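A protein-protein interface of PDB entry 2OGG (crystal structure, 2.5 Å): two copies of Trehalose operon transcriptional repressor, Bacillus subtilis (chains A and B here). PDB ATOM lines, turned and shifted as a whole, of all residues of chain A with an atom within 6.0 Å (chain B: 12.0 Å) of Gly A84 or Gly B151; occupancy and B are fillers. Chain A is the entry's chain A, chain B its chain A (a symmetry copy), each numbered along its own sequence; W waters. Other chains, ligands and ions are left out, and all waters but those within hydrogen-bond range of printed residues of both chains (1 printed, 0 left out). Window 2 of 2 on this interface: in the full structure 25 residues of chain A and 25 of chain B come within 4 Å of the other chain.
No position is printed for both chains. Of the 6 pairs that touch across the chains among the printed residues, none has its exchanged pair printed and touching as well.
OE2 of Glu A80 lies within salt-bridge range of NH2 of Arg B150 (3.1 Å). The backbone carbonyl oxygen (O) of Ser A88 lies within hydrogen-bond range of the backbone NH (N) of Arg B150 (2.8 Å).
Glu A80 touches just one residue of chain B: Arg B150. No residue of chain B comes within 4 Å of Leu A83. Of the printed residues of chain B, Gly A84 touches Gly B151. Leu A85 touches none of the printed residues of chain B. Of chain B, only Arg B150 (3.7 Å) and Gly B151 (3.6 Å) come within 4 Å of Ile A87. Ala B148 touches none of the printed residues of chain A. Of the printed residues of chain A, Arg B149 touches Ser A88 (3.6 Å). Printed residues of chain A within 4 Å of Arg B150: Glu A80 (3.1 Å), Ile A87 (3.7 Å) and Ser A88 (2.8 Å). Lys B152 touches none of the printed residues of chain A. The nearest residue of chain B that does not touch Gly A84 is Lys B152 (5.1 Å).
O of Gly A84 touches CA of Gly B151, 3.7 Å away. C of Arg B150 touches O of Ile A87 (3.7 Å). Gly B151 touches Ile A87 (N to O, 3.6 Å). Arg B149 touches Ser A88.
Water W1 lies within hydrogen-bond range of the side-chain carboxylate (OE1) of Glu A80, the backbone carbonyl oxygen (O) of Gly A84 and the backbone NH (N) of Gly B151.
Of the 10 printed residues of chain A, 4 touch a printed residue of chain B. Printed residues of chain A that touch a printed residue of chain B: Glu A80, Gly A84, Ile A87 and Ser A88. Hydrophobic or aromatic side chains of chain A within 4 Å of the printed part of chain B: Ile A87. Along chain A the printed residues that touch a printed residue of chain B span positions 80 to 88. Of the 6 printed residues of chain B, 3 touch a printed residue of chain A. Printed residues of chain B that touch a printed residue of chain A: Arg B149, Arg B150 and Gly B151. Along chain B the printed residues that touch a printed residue of chain A span positions 149 to 151. Among the printed residues, 6 pairs touch across the chains. Among the printed residues, Asp or Glu carboxylates within 4 Å of a Lys or Arg side-chain nitrogen of the other chain: Glu A80 with Arg B150.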
ATOM      1  N   ILE A  79       7.498  -3.187  -4.079  1.00  0.00           N
ATOM      2  CA  ILE A  79       7.385  -2.841  -2.668  1.00  0.00           C
ATOM      3  C   ILE A  79       6.854  -1.447  -2.405  1.00  0.00           C
ATOM      4  O   ILE A  79       5.902  -1.284  -1.667  1.00  0.00           O
ATOM      5  CB  ILE A  79       8.713  -3.069  -1.960  1.00  0.00           C
ATOM      6  CG1 ILE A  79       8.963  -4.574  -1.915  1.00  0.00           C
ATOM      7  CG2 ILE A  79       8.679  -2.488  -0.581  1.00  0.00           C
ATOM      8  CD1 ILE A  79      10.055  -4.990  -1.012  1.00  0.00           C
ATOM      9  N   GLU A  80       7.378  -0.455  -3.110  1.00  0.00           N
ATOM     10  CA  GLU A  80       6.833   0.889  -3.024  1.00  0.00           C
ATOM     11  C   GLU A  80       5.361   0.912  -3.429  1.00  0.00           C
ATOM     12  O   GLU A  80       4.545   1.628  -2.836  1.00  0.00           O
ATOM     13  CB  GLU A  80       7.622   1.826  -3.915  1.00  0.00           C
ATOM     14  CG  GLU A  80       9.030   2.111  -3.421  1.00  0.00           C
ATOM     15  CD  GLU A  80       9.025   2.901  -2.127  1.00  0.00           C
ATOM     16  OE1 GLU A  80       8.440   4.011  -2.109  1.00  0.00           O
ATOM     17  OE2 GLU A  80       9.594   2.403  -1.127  1.00  0.00           O
ATOM     18  N   GLY A  81       4.999   0.064  -4.382  1.00  0.00           N
ATOM     19  CA  GLY A  81       3.629   0.062  -4.872  1.00  0.00           C
ATOM     20  C   GLY A  81       2.657  -0.411  -3.811  1.00  0.00           C
ATOM     21  O   GLY A  81       1.531   0.097  -3.730  1.00  0.00           O
ATOM     22  N   GLU A  82       3.100  -1.367  -2.987  1.00  0.00           N
ATOM     23  CA  GLU A  82       2.245  -2.031  -1.993  1.00  0.00           C
ATOM     24  C   GLU A  82       2.228  -1.258  -0.706  1.00  0.00           C
ATOM     25  O   GLU A  82       1.211  -1.206  -0.050  1.00  0.00           O
ATOM     26  CB  GLU A  82       2.717  -3.459  -1.681  1.00  0.00           C
ATOM     27  CG  GLU A  82       2.626  -4.424  -2.858  1.00  0.00           C
ATOM     28  CD  GLU A  82       1.225  -4.498  -3.450  1.00  0.00           C
ATOM     29  OE1 GLU A  82       0.308  -4.898  -2.707  1.00  0.00           O
ATOM     30  OE2 GLU A  82       1.045  -4.171  -4.651  1.00  0.00           O
ATOM     31  N   LEU A  83       3.386  -0.757  -0.279  1.00  0.00           N
ATOM     32  CA  LEU A  83       3.456  -0.032   0.983  1.00  0.00           C
ATOM     33  C   LEU A  83       4.463   1.095   1.090  1.00  0.00           C
ATOM     34  O   LEU A  83       4.810   1.481   2.197  1.00  0.00           O
ATOM     35  CB  LEU A  83       3.555  -0.969   2.184  1.00  0.00           C
ATOM     36  CG  LEU A  83       4.560  -2.110   2.177  1.00  0.00           C
ATOM     37  CD1 LEU A  83       5.915  -1.551   2.019  1.00  0.00           C
ATOM     38  CD2 LEU A  83       4.454  -2.815   3.502  1.00  0.00           C
ATOM     39  N   GLY A  84       4.606   1.845   0.008  1.00  0.00           N
ATOM     40  CA  GLY A  84       5.562   2.937  -0.032  1.00  0.00           C
ATOM     41  C   GLY A  84       5.258   4.072   0.932  1.00  0.00           C
ATOM     42  O   GLY A  84       6.132   4.850   1.272  1.00  0.00           O
ATOM     43  N   LEU A  85       4.009   4.198   1.345  1.00  0.00           N
ATOM     44  CA  LEU A  85       3.596   5.328   2.187  1.00  0.00           C
ATOM     45  C   LEU A  85       3.927   5.012   3.665  1.00  0.00           C
ATOM     46  O   LEU A  85       3.982   5.902   4.505  1.00  0.00           O
ATOM     47  CB  LEU A  85       2.097   5.505   2.014  1.00  0.00           C
ATOM     48  CG  LEU A  85       1.353   6.837   1.943  1.00  0.00           C
ATOM     49  CD1 LEU A  85       2.036   7.873   1.035  1.00  0.00           C
ATOM     50  CD2 LEU A  85      -0.062   6.506   1.440  1.00  0.00           C
ATOM     51  N   SER A  86       4.220   3.745   3.953  1.00  0.00           N
ATOM     52  CA  SER A  86       4.508   3.300   5.313  1.00  0.00           C
ATOM     53  C   SER A  86       6.003   3.243   5.522  1.00  0.00           C
ATOM     54  O   SER A  86       6.461   2.897   6.602  1.00  0.00           O
ATOM     55  CB  SER A  86       3.959   1.894   5.539  1.00  0.00           C
ATOM     56  OG  SER A  86       2.571   1.821   5.295  1.00  0.00           O
ATOM     57  N   ILE A  87       6.749   3.295   4.428  1.00  0.00           N
ATOM     58  CA  ILE A  87       8.202   3.266   4.526  1.00  0.00           C
ATOM     59  C   ILE A  87       8.759   4.622   4.934  1.00  0.00           C
ATOM     60  O   ILE A  87       8.464   5.646   4.309  1.00  0.00           O
ATOM     61  CB  ILE A  87       8.849   2.823   3.215  1.00  0.00           C
ATOM     62  CG1 ILE A  87       8.274   1.467   2.793  1.00  0.00           C
ATOM     63  CG2 ILE A  87      10.378   2.742   3.394  1.00  0.00           C
ATOM     64  CD1 ILE A  87       9.075   0.767   1.699  1.00  0.00           C
ATOM     65  N   SER A  88       9.570   4.633   5.978  1.00  0.00           N
ATOM     66  CA  SER A  88       9.974   5.887   6.591  1.00  0.00           C
ATOM     67  C   SER A  88      11.379   6.333   6.212  1.00  0.00           C
ATOM     68  O   SER A  88      11.589   7.434   5.704  1.00  0.00           O
ATOM     69  CB  SER A  88       9.849   5.793   8.103  1.00  0.00           C
ATOM     70  OG  SER A  88      10.110   7.060   8.672  1.00  0.00           O
ATOM     71  N   PHE B 147      21.712   8.057   5.255  1.00  0.00           N
ATOM     72  CA  PHE B 147      20.316   7.933   4.869  1.00  0.00           C
ATOM     73  C   PHE B 147      20.309   8.818   3.623  1.00  0.00           C
ATOM     74  O   PHE B 147      21.328   9.459   3.344  1.00  0.00           O
ATOM     75  CB  PHE B 147      19.422   8.539   5.953  1.00  0.00           C
ATOM     76  CG  PHE B 147      19.891   8.265   7.348  1.00  0.00           C
ATOM     77  CD1 PHE B 147      20.857   9.057   7.932  1.00  0.00           C
ATOM     78  CD2 PHE B 147      19.273   7.303   8.117  1.00  0.00           C
ATOM     79  CE1 PHE B 147      21.272   8.829   9.232  1.00  0.00           C
ATOM     80  CE2 PHE B 147      19.674   7.060   9.422  1.00  0.00           C
ATOM     81  CZ  PHE B 147      20.688   7.816   9.975  1.00  0.00           C
ATOM     82  N   ALA B 148      19.274   8.766   2.785  1.00  0.00           N
ATOM     83  CA  ALA B 148      18.153   7.854   2.888  1.00  0.00           C
ATOM     84  C   ALA B 148      17.056   8.294   3.868  1.00  0.00           C
ATOM     85  O   ALA B 148      17.315   8.510   5.058  1.00  0.00           O
ATOM     86  CB  ALA B 148      18.625   6.426   3.142  1.00  0.00           C
ATOM     87  N   ARG B 149      15.966   8.765   3.272  1.00  0.00           N
ATOM     88  CA  ARG B 149      14.687   8.970   3.954  1.00  0.00           C
ATOM     89  C   ARG B 149      13.656   8.802   2.844  1.00  0.00           C
ATOM     90  O   ARG B 149      13.854   9.298   1.732  1.00  0.00           O
ATOM     91  CB  ARG B 149      14.589  10.374   4.556  1.00  0.00           C
ATOM     92  CG  ARG B 149      13.557  10.504   5.679  1.00  0.00           C
ATOM     93  CD  ARG B 149      14.119   9.984   7.004  1.00  0.00           C
ATOM     94  NE  ARG B 149      13.454  10.546   8.185  1.00  0.00           N
ATOM     95  CZ  ARG B 149      12.265  11.147   8.179  1.00  0.00           C
ATOM     96  NH1 ARG B 149      11.528  11.168   7.075  1.00  0.00           N
ATOM     97  NH2 ARG B 149      11.767  11.633   9.309  1.00  0.00           N
ATOM     98  N   ARG B 150      12.591   8.067   3.129  1.00  0.00           N
ATOM     99  CA  ARG B 150      11.708   7.567   2.085  1.00  0.00           C
ATOM    100  C   ARG B 150      10.278   8.105   2.229  1.00  0.00           C
ATOM    101  O   ARG B 150      10.007   8.907   3.118  1.00  0.00           O
ATOM    102  CB  ARG B 150      11.714   6.037   2.130  1.00  0.00           C
ATOM    103  CG  ARG B 150      13.116   5.415   2.133  1.00  0.00           C
ATOM    104  CD  ARG B 150      13.547   4.996   0.727  1.00  0.00           C
ATOM    105  NE  ARG B 150      12.767   3.857   0.230  1.00  0.00           N
ATOM    106  CZ  ARG B 150      13.255   2.632   0.048  1.00  0.00           C
ATOM    107  NH1 ARG B 150      14.557   2.411   0.179  1.00  0.00           N
ATOM    108  NH2 ARG B 150      12.462   1.661  -0.387  1.00  0.00           N
ATOM    109  N   GLY B 151       9.357   7.635   1.387  1.00  0.00           N
ATOM    110  CA  GLY B 151       7.965   8.076   1.458  1.00  0.00           C
ATOM    111  C   GLY B 151       7.743   9.358   0.684  1.00  0.00           C
ATOM    112  O   GLY B 151       8.677   9.902   0.085  1.00  0.00           O
ATOM    113  N   LYS B 152       6.524   9.886   0.769  1.00  0.00           N
ATOM    114  CA  LYS B 152       6.109  11.030  -0.056  1.00  0.00           C
ATOM    115  C   LYS B 152       7.006  12.262   0.146  1.00  0.00           C
ATOM    116  O   LYS B 152       7.248  13.109  -0.974  1.00  0.00           O
ATOM    117  CB  LYS B 152       4.627  11.364   0.185  1.00  0.00           C
ATOM    118  CG  LYS B 152       3.942  12.089  -0.959  1.00  0.00           C
ATOM    119  CD  LYS B 152       2.435  11.859  -0.931  1.00  0.00           C
ATOM    120  CE  LYS B 152       1.694  12.879  -0.073  1.00  0.00           C
ATOM    121  NZ  LYS B 152       1.334  14.118  -0.838  1.00  0.00           N
ATOM    122  OXT LYS B 152       7.594  12.417   1.384  1.00  0.00           O
HETATM  123  O   HOH W   1       8.706   4.939   0.381  1.00  0.00           O
